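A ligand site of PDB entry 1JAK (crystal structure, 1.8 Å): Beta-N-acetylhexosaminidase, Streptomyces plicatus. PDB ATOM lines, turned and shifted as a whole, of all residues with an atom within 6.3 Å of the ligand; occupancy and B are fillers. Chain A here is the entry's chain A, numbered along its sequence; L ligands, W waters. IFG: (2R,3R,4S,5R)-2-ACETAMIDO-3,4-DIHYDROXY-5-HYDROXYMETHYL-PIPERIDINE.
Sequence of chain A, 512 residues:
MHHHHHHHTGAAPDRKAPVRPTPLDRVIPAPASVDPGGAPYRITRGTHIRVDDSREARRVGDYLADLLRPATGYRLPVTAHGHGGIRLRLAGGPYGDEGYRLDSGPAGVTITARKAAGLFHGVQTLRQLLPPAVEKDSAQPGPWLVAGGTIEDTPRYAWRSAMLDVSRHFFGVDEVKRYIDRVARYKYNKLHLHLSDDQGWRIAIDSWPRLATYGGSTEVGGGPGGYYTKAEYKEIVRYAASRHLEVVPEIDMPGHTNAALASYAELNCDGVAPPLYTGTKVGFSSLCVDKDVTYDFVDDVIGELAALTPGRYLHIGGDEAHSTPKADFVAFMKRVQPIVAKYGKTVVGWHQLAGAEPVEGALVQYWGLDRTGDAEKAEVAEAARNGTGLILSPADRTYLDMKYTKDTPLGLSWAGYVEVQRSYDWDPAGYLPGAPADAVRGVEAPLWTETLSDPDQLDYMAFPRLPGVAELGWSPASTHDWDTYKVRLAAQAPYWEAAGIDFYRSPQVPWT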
ATOM      1  N   ASP A 165     -22.823  23.296  19.779  1.00  0.00           N
ATOM      2  CA  ASP A 165     -24.045  22.591  20.153  1.00  0.00           C
ATOM      3  C   ASP A 165     -23.891  22.222  21.639  1.00  0.00           C
ATOM      4  O   ASP A 165     -23.056  21.377  21.976  1.00  0.00           O
ATOM      5  CB  ASP A 165     -24.167  21.326  19.284  1.00  0.00           C
ATOM      6  CG  ASP A 165     -25.304  20.394  19.715  1.00  0.00           C
ATOM      7  OD1 ASP A 165     -26.040  20.676  20.683  1.00  0.00           O
ATOM      8  OD2 ASP A 165     -25.440  19.342  19.056  1.00  0.00           O
ATOM      9  N   ARG A 168     -26.870  18.552  22.677  1.00  0.00           N
ATOM     10  CA  ARG A 168     -26.608  17.106  22.632  1.00  0.00           C
ATOM     11  C   ARG A 168     -25.775  16.708  23.850  1.00  0.00           C
ATOM     12  O   ARG A 168     -26.067  15.710  24.505  1.00  0.00           O
ATOM     13  CB  ARG A 168     -25.933  16.744  21.307  1.00  0.00           C
ATOM     14  CG  ARG A 168     -26.938  16.525  20.174  1.00  0.00           C
ATOM     15  CD  ARG A 168     -28.072  17.570  20.159  1.00  0.00           C
ATOM     16  NE  ARG A 168     -29.033  17.305  19.094  1.00  0.00           N
ATOM     17  CZ  ARG A 168     -28.894  17.685  17.834  1.00  0.00           C
ATOM     18  NH1 ARG A 168     -27.830  18.391  17.455  1.00  0.00           N
ATOM     19  NH2 ARG A 168     -29.794  17.325  16.918  1.00  0.00           N
ATOM     20  N   HIS A 194     -26.332  26.733  19.985  1.00  0.00           N
ATOM     21  CA  HIS A 194     -27.510  25.891  19.770  1.00  0.00           C
ATOM     22  C   HIS A 194     -27.973  25.526  21.180  1.00  0.00           C
ATOM     23  O   HIS A 194     -27.534  24.521  21.754  1.00  0.00           O
ATOM     24  CB  HIS A 194     -27.108  24.639  18.976  1.00  0.00           C
ATOM     25  CG  HIS A 194     -28.263  23.865  18.432  1.00  0.00           C
ATOM     26  ND1 HIS A 194     -28.981  24.267  17.324  1.00  0.00           N
ATOM     27  CD2 HIS A 194     -28.808  22.691  18.835  1.00  0.00           C
ATOM     28  CE1 HIS A 194     -29.923  23.373  17.073  1.00  0.00           C
ATOM     29  NE2 HIS A 194     -29.844  22.414  17.963  1.00  0.00           N
ATOM     30  N   ASP A 197     -32.640  21.461  21.840  1.00  0.00           N
ATOM     31  CA  ASP A 197     -32.824  20.404  20.863  1.00  0.00           C
ATOM     32  C   ASP A 197     -33.605  19.283  21.531  1.00  0.00           C
ATOM     33  O   ASP A 197     -34.263  19.499  22.548  1.00  0.00           O
ATOM     34  CB  ASP A 197     -31.476  19.915  20.325  1.00  0.00           C
ATOM     35  CG  ASP A 197     -31.572  19.393  18.904  1.00  0.00           C
ATOM     36  OD1 ASP A 197     -32.134  18.303  18.713  1.00  0.00           O
ATOM     37  OD2 ASP A 197     -31.112  20.099  17.978  1.00  0.00           O
ATOM     38  N   ASP A 252     -34.362  26.122  18.479  1.00  0.00           N
ATOM     39  CA  ASP A 252     -34.871  25.428  17.305  1.00  0.00           C
ATOM     40  C   ASP A 252     -36.374  25.138  17.346  1.00  0.00           C
ATOM     41  O   ASP A 252     -36.889  24.649  18.344  1.00  0.00           O
ATOM     42  CB  ASP A 252     -34.102  24.112  17.126  1.00  0.00           C
ATOM     43  CG  ASP A 252     -33.974  23.699  15.675  1.00  0.00           C
ATOM     44  OD1 ASP A 252     -34.829  24.099  14.858  1.00  0.00           O
ATOM     45  OD2 ASP A 252     -33.027  22.943  15.355  1.00  0.00           O
ATOM     46  N   HIS A 256     -36.910  19.489  16.381  1.00  0.00           N
ATOM     47  CA  HIS A 256     -35.839  19.461  17.387  1.00  0.00           C
ATOM     48  C   HIS A 256     -36.290  20.098  18.684  1.00  0.00           C
ATOM     49  O   HIS A 256     -35.533  20.830  19.342  1.00  0.00           O
ATOM     50  CB  HIS A 256     -34.610  20.191  16.844  1.00  0.00           C
ATOM     51  CG  HIS A 256     -33.842  19.400  15.830  1.00  0.00           C
ATOM     52  ND1 HIS A 256     -33.007  18.360  16.181  1.00  0.00           N
ATOM     53  CD2 HIS A 256     -33.824  19.452  14.477  1.00  0.00           C
ATOM     54  CE1 HIS A 256     -32.509  17.810  15.089  1.00  0.00           C
ATOM     55  NE2 HIS A 256     -32.996  18.455  14.045  1.00  0.00           N
ATOM     56  N   THR A 280     -29.467   9.572  19.481  1.00  0.00           N
ATOM     57  CA  THR A 280     -28.740  10.443  18.559  1.00  0.00           C
ATOM     58  C   THR A 280     -29.400  10.604  17.188  1.00  0.00           C
ATOM     59  O   THR A 280     -28.734  10.976  16.213  1.00  0.00           O
ATOM     60  CB  THR A 280     -27.291   9.934  18.358  1.00  0.00           C
ATOM     61  OG1 THR A 280     -27.320   8.545  17.990  1.00  0.00           O
ATOM     62  CG2 THR A 280     -26.487  10.101  19.651  1.00  0.00           C
ATOM     63  N   LYS A 281     -30.699  10.343  17.107  1.00  0.00           N
ATOM     64  CA  LYS A 281     -31.406  10.502  15.848  1.00  0.00           C
ATOM     65  C   LYS A 281     -31.999  11.906  15.768  1.00  0.00           C
ATOM     66  O   LYS A 281     -31.954  12.658  16.757  1.00  0.00           O
ATOM     67  CB  LYS A 281     -32.527   9.459  15.732  1.00  0.00           C
ATOM     68  CG  LYS A 281     -32.013   8.042  15.483  1.00  0.00           C
ATOM     69  CD  LYS A 281     -33.160   7.031  15.432  1.00  0.00           C
ATOM     70  CE  LYS A 281     -34.232   7.433  14.428  1.00  0.00           C
ATOM     71  NZ  LYS A 281     -33.686   7.551  13.038  1.00  0.00           N
ATOM     72  N   VAL A 282     -32.524  12.273  14.603  1.00  0.00           N
ATOM     73  CA  VAL A 282     -33.125  13.581  14.390  1.00  0.00           C
ATOM     74  C   VAL A 282     -34.385  13.498  13.537  1.00  0.00           C
ATOM     75  O   VAL A 282     -34.596  12.519  12.822  1.00  0.00           O
ATOM     76  CB  VAL A 282     -32.160  14.561  13.659  1.00  0.00           C
ATOM     77  CG1 VAL A 282     -30.831  14.648  14.400  1.00  0.00           C
ATOM     78  CG2 VAL A 282     -31.942  14.116  12.207  1.00  0.00           C
ATOM     79  N   ASP A 319     -34.720  23.478  10.916  1.00  0.00           N
ATOM     80  CA  ASP A 319     -34.158  22.300  10.266  1.00  0.00           C
ATOM     81  C   ASP A 319     -34.825  20.999  10.673  1.00  0.00           C
ATOM     82  O   ASP A 319     -35.339  20.860  11.784  1.00  0.00           O
ATOM     83  CB  ASP A 319     -32.680  22.182  10.617  1.00  0.00           C
ATOM     84  CG  ASP A 319     -32.462  21.973  12.102  1.00  0.00           C
ATOM     85  OD1 ASP A 319     -32.903  22.845  12.882  1.00  0.00           O
ATOM     86  OD2 ASP A 319     -31.875  20.944  12.501  1.00  0.00           O
ATOM     87  N   GLU A 320     -34.786  20.035   9.755  1.00  0.00           N
ATOM     88  CA  GLU A 320     -35.291  18.706  10.005  1.00  0.00           C
ATOM     89  C   GLU A 320     -36.626  18.597  10.761  1.00  0.00           C
ATOM     90  O   GLU A 320     -36.752  17.798  11.691  1.00  0.00           O
ATOM     91  CB  GLU A 320     -34.187  17.916  10.737  1.00  0.00           C
ATOM     92  CG  GLU A 320     -32.855  17.975   9.990  1.00  0.00           C
ATOM     93  CD  GLU A 320     -31.681  17.415  10.780  1.00  0.00           C
ATOM     94  OE1 GLU A 320     -31.733  17.393  12.025  1.00  0.00           O
ATOM     95  OE2 GLU A 320     -30.681  17.016  10.151  1.00  0.00           O
ATOM     96  N   TRP A 350     -32.287  28.017   9.550  1.00  0.00           N
ATOM     97  CA  TRP A 350     -31.545  27.134   8.657  1.00  0.00           C
ATOM     98  C   TRP A 350     -32.213  27.325   7.298  1.00  0.00           C
ATOM     99  O   TRP A 350     -33.327  27.842   7.226  1.00  0.00           O
ATOM    100  CB  TRP A 350     -31.630  25.683   9.156  1.00  0.00           C
ATOM    101  CG  TRP A 350     -30.934  25.517  10.479  1.00  0.00           C
ATOM    102  CD1 TRP A 350     -31.510  25.424  11.710  1.00  0.00           C
ATOM    103  CD2 TRP A 350     -29.519  25.472  10.704  1.00  0.00           C
ATOM    104  NE1 TRP A 350     -30.548  25.331  12.684  1.00  0.00           N
ATOM    105  CE2 TRP A 350     -29.315  25.355  12.092  1.00  0.00           C
ATOM    106  CE3 TRP A 350     -28.394  25.509   9.855  1.00  0.00           C
ATOM    107  CZ2 TRP A 350     -28.031  25.275  12.670  1.00  0.00           C
ATOM    108  CZ3 TRP A 350     -27.114  25.431  10.416  1.00  0.00           C
ATOM    109  CH2 TRP A 350     -26.956  25.315  11.813  1.00  0.00           C
ATOM    110  N   GLN A 352     -34.005  25.712   5.425  1.00  0.00           N
ATOM    111  CA  GLN A 352     -35.342  25.174   5.194  1.00  0.00           C
ATOM    112  C   GLN A 352     -36.341  26.328   5.254  1.00  0.00           C
ATOM    113  O   GLN A 352     -37.440  26.249   4.703  1.00  0.00           O
ATOM    114  CB  GLN A 352     -35.713  24.138   6.270  1.00  0.00           C
ATOM    115  CG  GLN A 352     -35.099  22.758   6.067  1.00  0.00           C
ATOM    116  CD  GLN A 352     -33.584  22.777   6.121  1.00  0.00           C
ATOM    117  OE1 GLN A 352     -32.992  23.405   6.997  1.00  0.00           O
ATOM    118  NE2 GLN A 352     -32.943  22.073   5.190  1.00  0.00           N
ATOM    119  N   TRP A 367     -26.950  24.645   4.903  1.00  0.00           N
ATOM    120  CA  TRP A 367     -26.135  23.528   5.332  1.00  0.00           C
ATOM    121  C   TRP A 367     -26.226  22.353   4.358  1.00  0.00           C
ATOM    122  O   TRP A 367     -26.020  21.195   4.730  1.00  0.00           O
ATOM    123  CB  TRP A 367     -26.531  23.078   6.751  1.00  0.00           C
ATOM    124  CG  TRP A 367     -27.972  22.679   6.927  1.00  0.00           C
ATOM    125  CD1 TRP A 367     -29.072  23.502   6.901  1.00  0.00           C
ATOM    126  CD2 TRP A 367     -28.465  21.369   7.218  1.00  0.00           C
ATOM    127  NE1 TRP A 367     -30.208  22.769   7.154  1.00  0.00           N
ATOM    128  CE2 TRP A 367     -29.869  21.461   7.351  1.00  0.00           C
ATOM    129  CE3 TRP A 367     -27.849  20.109   7.382  1.00  0.00           C
ATOM    130  CZ2 TRP A 367     -30.677  20.348   7.648  1.00  0.00           C
ATOM    131  CZ3 TRP A 367     -28.655  19.010   7.679  1.00  0.00           C
ATOM    132  CH2 TRP A 367     -30.050  19.136   7.806  1.00  0.00           C
ATOM    133  N   TYR A 399     -19.003  21.356   8.641  1.00  0.00           N
ATOM    134  CA  TYR A 399     -19.571  20.729   9.819  1.00  0.00           C
ATOM    135  C   TYR A 399     -18.404  20.028  10.508  1.00  0.00           C
ATOM    136  O   TYR A 399     -17.911  19.003  10.039  1.00  0.00           O
ATOM    137  CB  TYR A 399     -20.655  19.722   9.409  1.00  0.00           C
ATOM    138  CG  TYR A 399     -22.053  20.313   9.400  1.00  0.00           C
ATOM    139  CD1 TYR A 399     -22.264  21.638   9.013  1.00  0.00           C
ATOM    140  CD2 TYR A 399     -23.156  19.563   9.806  1.00  0.00           C
ATOM    141  CE1 TYR A 399     -23.539  22.198   9.037  1.00  0.00           C
ATOM    142  CE2 TYR A 399     -24.435  20.109   9.830  1.00  0.00           C
ATOM    143  CZ  TYR A 399     -24.614  21.435   9.445  1.00  0.00           C
ATOM    144  OH  TYR A 399     -25.871  21.997   9.512  1.00  0.00           O
ATOM    145  N   ASP A 401     -18.243  18.276  13.112  1.00  0.00           N
ATOM    146  CA  ASP A 401     -18.538  16.992  13.732  1.00  0.00           C
ATOM    147  C   ASP A 401     -18.397  15.859  12.725  1.00  0.00           C
ATOM    148  O   ASP A 401     -18.459  14.681  13.088  1.00  0.00           O
ATOM    149  CB  ASP A 401     -19.957  16.974  14.309  1.00  0.00           C
ATOM    150  CG  ASP A 401     -21.025  17.133  13.240  1.00  0.00           C
ATOM    151  OD1 ASP A 401     -20.894  18.051  12.404  1.00  0.00           O
ATOM    152  OD2 ASP A 401     -21.979  16.336  13.220  1.00  0.00           O
ATOM    153  N   MET A 402     -18.198  16.199  11.456  1.00  0.00           N
ATOM    154  CA  MET A 402     -18.075  15.164  10.433  1.00  0.00           C
ATOM    155  C   MET A 402     -16.696  14.512  10.430  1.00  0.00           C
ATOM    156  O   MET A 402     -15.670  15.192  10.552  1.00  0.00           O
ATOM    157  CB  MET A 402     -18.381  15.740   9.048  1.00  0.00           C
ATOM    158  CG  MET A 402     -19.174  14.791   8.134  1.00  0.00           C
ATOM    159  SD  MET A 402     -20.799  14.349   8.825  1.00  0.00           S
ATOM    160  CE  MET A 402     -21.587  15.959   8.913  1.00  0.00           C
ATOM    161  N   LEU A 412     -19.564  12.079  12.987  1.00  0.00           N
ATOM    162  CA  LEU A 412     -20.558  11.397  12.164  1.00  0.00           C
ATOM    163  C   LEU A 412     -20.100  11.252  10.719  1.00  0.00           C
ATOM    164  O   LEU A 412     -19.109  11.858  10.305  1.00  0.00           O
ATOM    165  CB  LEU A 412     -21.893  12.140  12.222  1.00  0.00           C
ATOM    166  CG  LEU A 412     -22.494  12.299  13.622  1.00  0.00           C
ATOM    167  CD1 LEU A 412     -23.829  13.010  13.525  1.00  0.00           C
ATOM    168  CD2 LEU A 412     -22.676  10.920  14.265  1.00  0.00           C
ATOM    169  N   TRP A 414     -22.762  10.800   7.945  1.00  0.00           N
ATOM    170  CA  TRP A 414     -23.893  10.888   7.030  1.00  0.00           C
ATOM    171  C   TRP A 414     -23.667  11.811   5.837  1.00  0.00           C
ATOM    172  O   TRP A 414     -24.287  11.624   4.788  1.00  0.00           O
ATOM    173  CB  TRP A 414     -25.165  11.320   7.793  1.00  0.00           C
ATOM    174  CG  TRP A 414     -25.095  12.712   8.338  1.00  0.00           C
ATOM    175  CD1 TRP A 414     -24.682  13.091   9.582  1.00  0.00           C
ATOM    176  CD2 TRP A 414     -25.445  13.912   7.644  1.00  0.00           C
ATOM    177  NE1 TRP A 414     -24.751  14.462   9.713  1.00  0.00           N
ATOM    178  CE2 TRP A 414     -25.217  14.991   8.531  1.00  0.00           C
ATOM    179  CE3 TRP A 414     -25.926  14.195   6.355  1.00  0.00           C
ATOM    180  CZ2 TRP A 414     -25.446  16.326   8.175  1.00  0.00           C
ATOM    181  CZ3 TRP A 414     -26.168  15.524   6.003  1.00  0.00           C
ATOM    182  CH2 TRP A 414     -25.930  16.572   6.909  1.00  0.00           C
ATOM    183  N   TRP A 448     -21.408  20.124  16.049  1.00  0.00           N
ATOM    184  CA  TRP A 448     -22.503  19.389  16.671  1.00  0.00           C
ATOM    185  C   TRP A 448     -21.914  18.415  17.692  1.00  0.00           C
ATOM    186  O   TRP A 448     -20.808  17.914  17.502  1.00  0.00           O
ATOM    187  CB  TRP A 448     -23.310  18.648  15.598  1.00  0.00           C
ATOM    188  CG  TRP A 448     -23.903  19.621  14.620  1.00  0.00           C
ATOM    189  CD1 TRP A 448     -23.462  19.900  13.355  1.00  0.00           C
ATOM    190  CD2 TRP A 448     -25.036  20.465  14.842  1.00  0.00           C
ATOM    191  NE1 TRP A 448     -24.249  20.878  12.784  1.00  0.00           N
ATOM    192  CE2 TRP A 448     -25.224  21.243  13.680  1.00  0.00           C
ATOM    193  CE3 TRP A 448     -25.915  20.649  15.924  1.00  0.00           C
ATOM    194  CZ2 TRP A 448     -26.251  22.177  13.562  1.00  0.00           C
ATOM    195  CZ3 TRP A 448     -26.932  21.581  15.808  1.00  0.00           C
ATOM    196  CH2 TRP A 448     -27.099  22.333  14.632  1.00  0.00           C
ATOM    197  N   GLU A 450     -23.367  15.300  19.183  1.00  0.00           N
ATOM    198  CA  GLU A 450     -23.931  13.975  19.453  1.00  0.00           C
ATOM    199  C   GLU A 450     -22.852  13.028  19.967  1.00  0.00           C
ATOM    200  O   GLU A 450     -23.123  12.180  20.816  1.00  0.00           O
ATOM    201  CB  GLU A 450     -24.533  13.358  18.187  1.00  0.00           C
ATOM    202  CG  GLU A 450     -25.946  13.802  17.867  1.00  0.00           C
ATOM    203  CD  GLU A 450     -26.010  15.010  16.952  1.00  0.00           C
ATOM    204  OE1 GLU A 450     -24.990  15.726  16.818  1.00  0.00           O
ATOM    205  OE2 GLU A 450     -27.089  15.246  16.366  1.00  0.00           O
HETATM  206  N1  IFG L   1     -28.238  17.869  11.225  1.00  0.00           N
HETATM  207  C2  IFG L   1     -28.901  18.550  12.379  1.00  0.00           C
HETATM  208  C3  IFG L   1     -27.990  18.784  13.645  1.00  0.00           C
HETATM  209  C4  IFG L   1     -27.027  17.620  13.952  1.00  0.00           C
HETATM  210  C5  IFG L   1     -26.242  17.294  12.675  1.00  0.00           C
HETATM  211  C6  IFG L   1     -25.204  16.185  12.818  1.00  0.00           C
HETATM  212  C7  IFG L   1     -28.662  20.722  11.251  1.00  0.00           C
HETATM  213  C8  IFG L   1     -29.106  22.086  10.782  1.00  0.00           C
HETATM  214  C9  IFG L   1     -27.159  16.915  11.502  1.00  0.00           C
HETATM  215  N2  IFG L   1     -29.458  19.849  11.921  1.00  0.00           N
HETATM  216  O7  IFG L   1     -27.504  20.421  10.988  1.00  0.00           O
HETATM  217  O3  IFG L   1     -28.820  19.022  14.777  1.00  0.00           O
HETATM  218  O4  IFG L   1     -27.802  16.477  14.326  1.00  0.00           O
HETATM  219  O6  IFG L   1     -24.205  16.286  11.801  1.00  0.00           O
HETATM  220  O   HOH W   1     -30.616  20.942  15.064  1.00  0.00           O
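OE2 of Glu 450 lies within hydrogen-bond range of O4 of the ligand, 2.5 Å away.
OD2 of Asp 401 is in hydrogen-bond range of O6 of the ligand (2.6 Å).
OH of Tyr 399 lies within hydrogen-bond range of O7 of the ligand (2.7 Å).
A nitrogen (N2) of the ligand is in hydrogen-bond range of the side-chain carboxylate (OD2) of Asp 319, 2.7 Å away.
A nitrogen (N1) of the ligand is in salt-bridge range of the side-chain carboxylate of Glu 320, 2.8 Å away.
NE1 of Trp 414 sits at hydrogen-bond distance from O6 of the ligand, 2.8 Å away.
The guanidinium group of Arg 168 lies within hydrogen-bond range of an oxygen (O3) of the ligand, 2.9 Å away.
The backbone carbonyl oxygen of Asp 401 is in hydrogen-bond range of the backbone NH of Leu 412 (2.8 Å).
NE1 of Trp 350 lies close to OD1 of Asp 319 (3.4 Å).
A ring nitrogen (NE2) of His 256 lies within hydrogen-bond range of the side-chain carboxylate (OD2) of Asp 319 (3.1 Å).
The side-chain carboxylate (OD2) of Asp 252 lies close to the side-chain carboxylate (OD1) of Asp 319 (2.5 Å).
A ring nitrogen (NE2) of His 256 sits at hydrogen-bond distance from the side-chain carboxylate (OE1) of Glu 320 (2.6 Å).
A ring nitrogen (ND1) of His 256 sits close to the guanidinium group (NH2) of Arg 168.
The side-chain carboxylate (OD1) of Asp 197 is in salt-bridge range of the guanidinium group (NH2) of Arg 168, 3.1 Å away.
NH1 of Arg 168 is in salt-bridge range of OD2 of Asp 165 (3.0 Å).
CE1 of His 256 touches O3 of the ligand, at 3.9 Å.
Val 282 touches the ligand.
Trp 350 touches the ligand (CD2 to C8, 3.4 Å).
CE2 of Trp 367 touches C8 of the ligand, at 3.6 Å.
Met 402 touches the ligand (CE to O6, 3.9 Å).
Leu 412 touches the ligand (CD1 to C6, 3.5 Å).
Trp 448 touches the ligand.
Hydrophobic or aromatic side chains that line the ligand: His 256, Val 282, Trp 350, Trp 367, Tyr 399, Met 402, Leu 412, Trp 414 and Trp 448.
The nearest printed residue that does not touch the ligand is Asp 197 (4.1 Å).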
